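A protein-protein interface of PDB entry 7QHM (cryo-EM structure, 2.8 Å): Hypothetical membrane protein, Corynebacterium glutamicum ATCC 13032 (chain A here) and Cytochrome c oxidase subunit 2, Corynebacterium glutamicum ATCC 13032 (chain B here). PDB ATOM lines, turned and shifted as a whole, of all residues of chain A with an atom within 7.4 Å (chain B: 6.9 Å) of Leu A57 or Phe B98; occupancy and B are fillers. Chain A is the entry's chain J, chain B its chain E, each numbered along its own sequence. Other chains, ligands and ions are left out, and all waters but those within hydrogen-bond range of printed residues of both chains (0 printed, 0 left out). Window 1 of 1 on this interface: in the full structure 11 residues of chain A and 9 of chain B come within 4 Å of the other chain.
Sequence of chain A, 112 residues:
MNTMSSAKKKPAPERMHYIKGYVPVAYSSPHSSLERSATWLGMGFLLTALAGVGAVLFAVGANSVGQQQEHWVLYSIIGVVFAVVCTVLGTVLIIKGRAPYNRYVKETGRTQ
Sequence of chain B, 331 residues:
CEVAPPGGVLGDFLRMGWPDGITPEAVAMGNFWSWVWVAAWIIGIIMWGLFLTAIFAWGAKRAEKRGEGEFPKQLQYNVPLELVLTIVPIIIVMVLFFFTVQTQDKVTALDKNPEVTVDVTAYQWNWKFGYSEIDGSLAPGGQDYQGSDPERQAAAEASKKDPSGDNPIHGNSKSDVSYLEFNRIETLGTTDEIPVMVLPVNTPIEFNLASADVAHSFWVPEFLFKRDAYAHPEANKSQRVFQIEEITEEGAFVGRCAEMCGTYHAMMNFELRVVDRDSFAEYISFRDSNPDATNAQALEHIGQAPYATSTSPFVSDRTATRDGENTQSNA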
ATOM      1  N   LEU A  50      -7.714 -10.508 -31.223  1.00  0.00           N
ATOM      2  CA  LEU A  50      -8.702 -11.343 -30.550  1.00  0.00           C
ATOM      3  C   LEU A  50     -10.009 -11.454 -31.326  1.00  0.00           C
ATOM      4  O   LEU A  50     -10.778 -12.394 -31.095  1.00  0.00           O
ATOM      5  CB  LEU A  50      -8.982 -10.792 -29.157  1.00  0.00           C
ATOM      6  CG  LEU A  50      -7.800 -10.660 -28.203  1.00  0.00           C
ATOM      7  CD1 LEU A  50      -8.218  -9.851 -26.989  1.00  0.00           C
ATOM      8  CD2 LEU A  50      -7.293 -12.024 -27.777  1.00  0.00           C
ATOM      9  N   ALA A  51     -10.289 -10.521 -32.233  1.00  0.00           N
ATOM     10  CA  ALA A  51     -11.499 -10.638 -33.032  1.00  0.00           C
ATOM     11  C   ALA A  51     -11.436 -11.861 -33.938  1.00  0.00           C
ATOM     12  O   ALA A  51     -12.452 -12.532 -34.160  1.00  0.00           O
ATOM     13  CB  ALA A  51     -11.713  -9.366 -33.849  1.00  0.00           C
ATOM     14  N   GLY A  52     -10.250 -12.177 -34.453  1.00  0.00           N
ATOM     15  CA  GLY A  52     -10.104 -13.389 -35.238  1.00  0.00           C
ATOM     16  C   GLY A  52     -10.395 -14.636 -34.427  1.00  0.00           C
ATOM     17  O   GLY A  52     -11.060 -15.556 -34.903  1.00  0.00           O
ATOM     18  N   VAL A  53      -9.905 -14.679 -33.188  1.00  0.00           N
ATOM     19  CA  VAL A  53     -10.141 -15.841 -32.339  1.00  0.00           C
ATOM     20  C   VAL A  53     -11.620 -15.958 -32.012  1.00  0.00           C
ATOM     21  O   VAL A  53     -12.173 -17.064 -31.927  1.00  0.00           O
ATOM     22  CB  VAL A  53      -9.286 -15.748 -31.063  1.00  0.00           C
ATOM     23  CG1 VAL A  53      -9.469 -16.999 -30.204  1.00  0.00           C
ATOM     24  CG2 VAL A  53      -7.813 -15.551 -31.412  1.00  0.00           C
ATOM     25  N   GLY A  54     -12.280 -14.819 -31.804  1.00  0.00           N
ATOM     26  CA  GLY A  54     -13.723 -14.836 -31.657  1.00  0.00           C
ATOM     27  C   GLY A  54     -14.405 -15.434 -32.868  1.00  0.00           C
ATOM     28  O   GLY A  54     -15.325 -16.243 -32.737  1.00  0.00           O
ATOM     29  N   ALA A  55     -13.941 -15.062 -34.066  1.00  0.00           N
ATOM     30  CA  ALA A  55     -14.531 -15.595 -35.291  1.00  0.00           C
ATOM     31  C   ALA A  55     -14.312 -17.095 -35.404  1.00  0.00           C
ATOM     32  O   ALA A  55     -15.190 -17.828 -35.875  1.00  0.00           O
ATOM     33  CB  ALA A  55     -13.946 -14.883 -36.505  1.00  0.00           C
ATOM     34  N   VAL A  56     -13.148 -17.575 -34.974  1.00  0.00           N
ATOM     35  CA  VAL A  56     -12.870 -19.007 -35.052  1.00  0.00           C
ATOM     36  C   VAL A  56     -13.783 -19.773 -34.107  1.00  0.00           C
ATOM     37  O   VAL A  56     -14.399 -20.772 -34.495  1.00  0.00           O
ATOM     38  CB  VAL A  56     -11.391 -19.298 -34.749  1.00  0.00           C
ATOM     39  CG1 VAL A  56     -11.150 -20.799 -34.683  1.00  0.00           C
ATOM     40  CG2 VAL A  56     -10.510 -18.692 -35.814  1.00  0.00           C
ATOM     41  N   LEU A  57     -13.851 -19.343 -32.844  1.00  0.00           N
ATOM     42  CA  LEU A  57     -14.751 -19.998 -31.902  1.00  0.00           C
ATOM     43  C   LEU A  57     -16.183 -19.961 -32.410  1.00  0.00           C
ATOM     44  O   LEU A  57     -16.902 -20.962 -32.321  1.00  0.00           O
ATOM     45  CB  LEU A  57     -14.662 -19.343 -30.525  1.00  0.00           C
ATOM     46  CG  LEU A  57     -13.333 -19.456 -29.785  1.00  0.00           C
ATOM     47  CD1 LEU A  57     -13.328 -18.568 -28.565  1.00  0.00           C
ATOM     48  CD2 LEU A  57     -13.054 -20.884 -29.378  1.00  0.00           C
ATOM     49  N   PHE A  58     -16.605 -18.828 -32.976  1.00  0.00           N
ATOM     50  CA  PHE A  58     -17.955 -18.726 -33.508  1.00  0.00           C
ATOM     51  C   PHE A  58     -18.201 -19.765 -34.588  1.00  0.00           C
ATOM     52  O   PHE A  58     -19.183 -20.510 -34.532  1.00  0.00           O
ATOM     53  CB  PHE A  58     -18.201 -17.330 -34.069  1.00  0.00           C
ATOM     54  CG  PHE A  58     -19.351 -17.269 -35.024  1.00  0.00           C
ATOM     55  CD1 PHE A  58     -20.648 -17.283 -34.559  1.00  0.00           C
ATOM     56  CD2 PHE A  58     -19.138 -17.211 -36.386  1.00  0.00           C
ATOM     57  CE1 PHE A  58     -21.706 -17.241 -35.435  1.00  0.00           C
ATOM     58  CE2 PHE A  58     -20.192 -17.170 -37.262  1.00  0.00           C
ATOM     59  CZ  PHE A  58     -21.476 -17.181 -36.788  1.00  0.00           C
ATOM     60  N   ALA A  59     -17.333 -19.811 -35.598  1.00  0.00           N
ATOM     61  CA  ALA A  59     -17.561 -20.710 -36.724  1.00  0.00           C
ATOM     62  C   ALA A  59     -17.533 -22.162 -36.277  1.00  0.00           C
ATOM     63  O   ALA A  59     -18.415 -22.953 -36.637  1.00  0.00           O
ATOM     64  CB  ALA A  59     -16.519 -20.460 -37.810  1.00  0.00           C
ATOM     65  N   VAL A  60     -16.528 -22.528 -35.477  1.00  0.00           N
ATOM     66  CA  VAL A  60     -16.418 -23.902 -34.995  1.00  0.00           C
ATOM     67  C   VAL A  60     -17.654 -24.283 -34.191  1.00  0.00           C
ATOM     68  O   VAL A  60     -18.273 -25.321 -34.437  1.00  0.00           O
ATOM     69  CB  VAL A  60     -15.130 -24.076 -34.173  1.00  0.00           C
ATOM     70  CG1 VAL A  60     -15.081 -25.448 -33.510  1.00  0.00           C
ATOM     71  CG2 VAL A  60     -13.917 -23.885 -35.060  1.00  0.00           C
ATOM     72  N   GLY A  61     -18.041 -23.446 -33.223  1.00  0.00           N
ATOM     73  CA  GLY A  61     -19.157 -23.791 -32.363  1.00  0.00           C
ATOM     74  C   GLY A  61     -20.497 -23.779 -33.069  1.00  0.00           C
ATOM     75  O   GLY A  61     -21.408 -24.514 -32.682  1.00  0.00           O
ATOM     76  N   ALA A  62     -20.641 -22.951 -34.100  1.00  0.00           N
ATOM     77  CA  ALA A  62     -21.877 -22.929 -34.862  1.00  0.00           C
ATOM     78  C   ALA A  62     -21.981 -24.132 -35.781  1.00  0.00           C
ATOM     79  O   ALA A  62     -23.083 -24.641 -36.002  1.00  0.00           O
ATOM     80  CB  ALA A  62     -21.972 -21.637 -35.670  1.00  0.00           C
ATOM     81  N   ASN A  63     -20.850 -24.606 -36.309  1.00  0.00           N
ATOM     82  CA  ASN A  63     -20.864 -25.870 -37.035  1.00  0.00           C
ATOM     83  C   ASN A  63     -21.042 -27.051 -36.098  1.00  0.00           C
ATOM     84  O   ASN A  63     -21.580 -28.084 -36.506  1.00  0.00           O
ATOM     85  CB  ASN A  63     -19.580 -26.034 -37.836  1.00  0.00           C
ATOM     86  CG  ASN A  63     -19.567 -27.309 -38.650  1.00  0.00           C
ATOM     87  OD1 ASN A  63     -20.381 -27.487 -39.555  1.00  0.00           O
ATOM     88  ND2 ASN A  63     -18.636 -28.206 -38.338  1.00  0.00           N
ATOM     89  N   SER A  64     -20.604 -26.919 -34.845  1.00  0.00           N
ATOM     90  CA  SER A  64     -20.639 -28.044 -33.920  1.00  0.00           C
ATOM     91  C   SER A  64     -22.066 -28.469 -33.612  1.00  0.00           C
ATOM     92  O   SER A  64     -22.325 -29.660 -33.418  1.00  0.00           O
ATOM     93  CB  SER A  64     -19.899 -27.679 -32.635  1.00  0.00           C
ATOM     94  OG  SER A  64     -19.879 -28.768 -31.729  1.00  0.00           O
ATOM     95  N   VAL A  65     -22.996 -27.519 -33.579  1.00  0.00           N
ATOM     96  CA  VAL A  65     -24.395 -27.797 -33.289  1.00  0.00           C
ATOM     97  C   VAL A  65     -25.230 -27.909 -34.560  1.00  0.00           C
ATOM     98  O   VAL A  65     -26.463 -27.886 -34.490  1.00  0.00           O
ATOM     99  CB  VAL A  65     -24.982 -26.739 -32.340  1.00  0.00           C
ATOM    100  CG1 VAL A  65     -24.262 -26.771 -31.000  1.00  0.00           C
ATOM    101  CG2 VAL A  65     -24.917 -25.342 -32.937  1.00  0.00           C
ATOM    102  N   SER A  76     -14.087 -19.605 -40.402  1.00  0.00           N
ATOM    103  CA  SER A  76     -12.965 -20.053 -39.589  1.00  0.00           C
ATOM    104  C   SER A  76     -11.626 -19.686 -40.231  1.00  0.00           C
ATOM    105  O   SER A  76     -10.680 -19.305 -39.529  1.00  0.00           O
ATOM    106  CB  SER A  76     -13.071 -21.559 -39.359  1.00  0.00           C
ATOM    107  OG  SER A  76     -12.271 -21.967 -38.264  1.00  0.00           O
ATOM    108  N   GLY A  79     -10.998 -16.046 -39.815  1.00  0.00           N
ATOM    109  CA  GLY A  79     -10.675 -15.815 -38.419  1.00  0.00           C
ATOM    110  C   GLY A  79      -9.231 -16.140 -38.087  1.00  0.00           C
ATOM    111  O   GLY A  79      -8.544 -15.357 -37.426  1.00  0.00           O
ATOM    112  N   PHE B  32     -27.133 -24.191 -19.225  1.00  0.00           N
ATOM    113  CA  PHE B  32     -26.025 -23.246 -19.349  1.00  0.00           C
ATOM    114  C   PHE B  32     -26.039 -22.241 -18.203  1.00  0.00           C
ATOM    115  O   PHE B  32     -24.984 -21.878 -17.666  1.00  0.00           O
ATOM    116  CB  PHE B  32     -26.100 -22.536 -20.700  1.00  0.00           C
ATOM    117  CG  PHE B  32     -25.018 -21.523 -20.919  1.00  0.00           C
ATOM    118  CD1 PHE B  32     -23.693 -21.903 -20.964  1.00  0.00           C
ATOM    119  CD2 PHE B  32     -25.330 -20.190 -21.105  1.00  0.00           C
ATOM    120  CE1 PHE B  32     -22.695 -20.968 -21.171  1.00  0.00           C
ATOM    121  CE2 PHE B  32     -24.337 -19.253 -21.314  1.00  0.00           C
ATOM    122  CZ  PHE B  32     -23.021 -19.643 -21.345  1.00  0.00           C
ATOM    123  N   VAL B  93     -12.876 -16.684 -20.438  1.00  0.00           N
ATOM    124  CA  VAL B  93     -13.862 -16.025 -21.284  1.00  0.00           C
ATOM    125  C   VAL B  93     -14.019 -16.757 -22.608  1.00  0.00           C
ATOM    126  O   VAL B  93     -15.107 -16.774 -23.192  1.00  0.00           O
ATOM    127  CB  VAL B  93     -13.449 -14.549 -21.474  1.00  0.00           C
ATOM    128  CG1 VAL B  93     -14.008 -13.964 -22.755  1.00  0.00           C
ATOM    129  CG2 VAL B  93     -13.889 -13.733 -20.274  1.00  0.00           C
ATOM    130  N   MET B  94     -12.948 -17.359 -23.110  1.00  0.00           N
ATOM    131  CA  MET B  94     -13.045 -18.039 -24.396  1.00  0.00           C
ATOM    132  C   MET B  94     -13.940 -19.270 -24.303  1.00  0.00           C
ATOM    133  O   MET B  94     -14.766 -19.509 -25.193  1.00  0.00           O
ATOM    134  CB  MET B  94     -11.651 -18.411 -24.893  1.00  0.00           C
ATOM    135  CG  MET B  94     -10.897 -17.237 -25.482  1.00  0.00           C
ATOM    136  SD  MET B  94      -9.192 -17.626 -25.911  1.00  0.00           S
ATOM    137  CE  MET B  94      -8.705 -16.105 -26.719  1.00  0.00           C
ATOM    138  N   VAL B  95     -13.804 -20.057 -23.234  1.00  0.00           N
ATOM    139  CA  VAL B  95     -14.685 -21.210 -23.077  1.00  0.00           C
ATOM    140  C   VAL B  95     -16.115 -20.753 -22.816  1.00  0.00           C
ATOM    141  O   VAL B  95     -17.075 -21.365 -23.311  1.00  0.00           O
ATOM    142  CB  VAL B  95     -14.177 -22.161 -21.976  1.00  0.00           C
ATOM    143  CG1 VAL B  95     -12.898 -22.848 -22.421  1.00  0.00           C
ATOM    144  CG2 VAL B  95     -13.964 -21.460 -20.645  1.00  0.00           C
ATOM    145  N   LEU B  96     -16.281 -19.670 -22.044  1.00  0.00           N
ATOM    146  CA  LEU B  96     -17.611 -19.098 -21.858  1.00  0.00           C
ATOM    147  C   LEU B  96     -18.255 -18.771 -23.198  1.00  0.00           C
ATOM    148  O   LEU B  96     -19.416 -19.114 -23.442  1.00  0.00           O
ATOM    149  CB  LEU B  96     -17.519 -17.848 -20.985  1.00  0.00           C
ATOM    150  CG  LEU B  96     -18.800 -17.066 -20.690  1.00  0.00           C
ATOM    151  CD1 LEU B  96     -19.819 -17.924 -19.964  1.00  0.00           C
ATOM    152  CD2 LEU B  96     -18.480 -15.818 -19.876  1.00  0.00           C
ATOM    153  N   PHE B  97     -17.493 -18.159 -24.103  1.00  0.00           N
ATOM    154  CA  PHE B  97     -18.054 -17.752 -25.385  1.00  0.00           C
ATOM    155  C   PHE B  97     -18.294 -18.943 -26.301  1.00  0.00           C
ATOM    156  O   PHE B  97     -19.241 -18.931 -27.093  1.00  0.00           O
ATOM    157  CB  PHE B  97     -17.134 -16.738 -26.055  1.00  0.00           C
ATOM    158  CG  PHE B  97     -17.546 -16.379 -27.449  1.00  0.00           C
ATOM    159  CD1 PHE B  97     -18.786 -15.821 -27.696  1.00  0.00           C
ATOM    160  CD2 PHE B  97     -16.690 -16.588 -28.512  1.00  0.00           C
ATOM    161  CE1 PHE B  97     -19.168 -15.487 -28.976  1.00  0.00           C
ATOM    162  CE2 PHE B  97     -17.069 -16.253 -29.795  1.00  0.00           C
ATOM    163  CZ  PHE B  97     -18.312 -15.703 -30.026  1.00  0.00           C
ATOM    164  N   PHE B  98     -17.463 -19.979 -26.217  1.00  0.00           N
ATOM    165  CA  PHE B  98     -17.697 -21.158 -27.043  1.00  0.00           C
ATOM    166  C   PHE B  98     -19.005 -21.836 -26.659  1.00  0.00           C
ATOM    167  O   PHE B  98     -19.850 -22.137 -27.521  1.00  0.00           O
ATOM    168  CB  PHE B  98     -16.537 -22.137 -26.916  1.00  0.00           C
ATOM    169  CG  PHE B  98     -16.633 -23.293 -27.856  1.00  0.00           C
ATOM    170  CD1 PHE B  98     -16.320 -23.135 -29.190  1.00  0.00           C
ATOM    171  CD2 PHE B  98     -17.048 -24.530 -27.412  1.00  0.00           C
ATOM    172  CE1 PHE B  98     -16.412 -24.188 -30.060  1.00  0.00           C
ATOM    173  CE2 PHE B  98     -17.141 -25.588 -28.279  1.00  0.00           C
ATOM    174  CZ  PHE B  98     -16.823 -25.418 -29.606  1.00  0.00           C
ATOM    175  N   PHE B  99     -19.201 -22.069 -25.361  1.00  0.00           N
ATOM    176  CA  PHE B  99     -20.468 -22.652 -24.941  1.00  0.00           C
ATOM    177  C   PHE B  99     -21.634 -21.702 -25.192  1.00  0.00           C
ATOM    178  O   PHE B  99     -22.756 -22.158 -25.450  1.00  0.00           O
ATOM    179  CB  PHE B  99     -20.389 -23.061 -23.478  1.00  0.00           C
ATOM    180  CG  PHE B  99     -19.497 -24.236 -23.239  1.00  0.00           C
ATOM    181  CD1 PHE B  99     -19.867 -25.497 -23.661  1.00  0.00           C
ATOM    182  CD2 PHE B  99     -18.292 -24.085 -22.590  1.00  0.00           C
ATOM    183  CE1 PHE B  99     -19.049 -26.583 -23.444  1.00  0.00           C
ATOM    184  CE2 PHE B  99     -17.468 -25.167 -22.368  1.00  0.00           C
ATOM    185  CZ  PHE B  99     -17.849 -26.418 -22.795  1.00  0.00           C
ATOM    186  N   THR B 100     -21.394 -20.388 -25.157  1.00  0.00           N
ATOM    187  CA  THR B 100     -22.444 -19.441 -25.510  1.00  0.00           C
ATOM    188  C   THR B 100     -22.882 -19.625 -26.955  1.00  0.00           C
ATOM    189  O   THR B 100     -24.082 -19.651 -27.249  1.00  0.00           O
ATOM    190  CB  THR B 100     -21.963 -18.007 -25.284  1.00  0.00           C
ATOM    191  OG1 THR B 100     -21.808 -17.765 -23.883  1.00  0.00           O
ATOM    192  CG2 THR B 100     -22.946 -17.001 -25.866  1.00  0.00           C
ATOM    193  N   VAL B 101     -21.918 -19.717 -27.876  1.00  0.00           N
ATOM    194  CA  VAL B 101     -22.248 -19.900 -29.288  1.00  0.00           C
ATOM    195  C   VAL B 101     -23.045 -21.180 -29.475  1.00  0.00           C
ATOM    196  O   VAL B 101     -24.058 -21.204 -30.187  1.00  0.00           O
ATOM    197  CB  VAL B 101     -20.962 -19.901 -30.137  1.00  0.00           C
ATOM    198  CG1 VAL B 101     -21.225 -20.407 -31.551  1.00  0.00           C
ATOM    199  CG2 VAL B 101     -20.370 -18.510 -30.187  1.00  0.00           C
ATOM    200  N   GLN B 102     -22.614 -22.259 -28.811  1.00  0.00           N
ATOM    201  CA  GLN B 102     -23.327 -23.528 -28.898  1.00  0.00           C
ATOM    202  C   GLN B 102     -24.778 -23.386 -28.462  1.00  0.00           C
ATOM    203  O   GLN B 102     -25.703 -23.711 -29.217  1.00  0.00           O
ATOM    204  CB  GLN B 102     -22.621 -24.574 -28.043  1.00  0.00           C
ATOM    205  CG  GLN B 102     -21.321 -25.068 -28.621  1.00  0.00           C
ATOM    206  CD  GLN B 102     -20.707 -26.162 -27.778  1.00  0.00           C
ATOM    207  OE1 GLN B 102     -20.499 -25.990 -26.579  1.00  0.00           O
ATOM    208  NE2 GLN B 102     -20.424 -27.303 -28.396  1.00  0.00           N
ATOM    209  N   THR B 103     -24.996 -22.900 -27.239  1.00  0.00           N
ATOM    210  CA  THR B 103     -26.351 -22.834 -26.695  1.00  0.00           C
ATOM    211  C   THR B 103     -27.228 -21.887 -27.506  1.00  0.00           C
ATOM    212  O   THR B 103     -28.404 -22.179 -27.762  1.00  0.00           O
ATOM    213  CB  THR B 103     -26.299 -22.393 -25.233  1.00  0.00           C
ATOM    214  OG1 THR B 103     -25.302 -23.143 -24.534  1.00  0.00           O
ATOM    215  CG2 THR B 103     -27.639 -22.605 -24.560  1.00  0.00           C
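Val A53 touches Met B94 (CG1 to CE, 3.7 Å).
Gly A54 touches Phe B97.
Leu A57 touches Phe B97 (CD1 to CD2, 3.9 Å).
Leu A57 touches Phe B98.
O of Phe A58 touches CG1 of Val B101, at 3.6 Å.
CE1 of Phe B98 touches CG1 of Val A60 (3.9 Å).
Phe B98 touches Gly A61.
Gly A61 touches Val B101 (C to CG1, 3.8 Å).
OG of Ser A64 touches NE2 of Gln B102, 3.7 Å away.
CG1 of Val A65 touches O of Gln B102, 3.8 Å away.
Leu A57 touches just these residues of chain B: Met B94, Phe B97 and Phe B98.
Of the printed residues of chain B, Ala A62 touches Val B101.
Of the printed residues of chain A, Phe B97 touches Gly A54 and Leu A57.
Of chain A, only Leu A57 (3.9 Å), Val A60 (3.9 Å) and Gly A61 (3.6 Å) come within 4 Å of Phe B98.
Of the printed residues of chain A, Val B101 touches Phe A58, Gly A61 and Ala A62.
The nearest residue of chain A that does not touch Phe B98 is Ser A64 (4.9 Å).
The nearest printed residue of chain B that does not touch Ser A64 is Phe B98 (4.9 Å).
Of the 18 printed residues of chain A, 9 touch a printed residue of chain B.
Hydrophobic or aromatic side chains of chain A that line the printed part of chain B: Val A53, Leu A57, Val A60 and Val A65.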
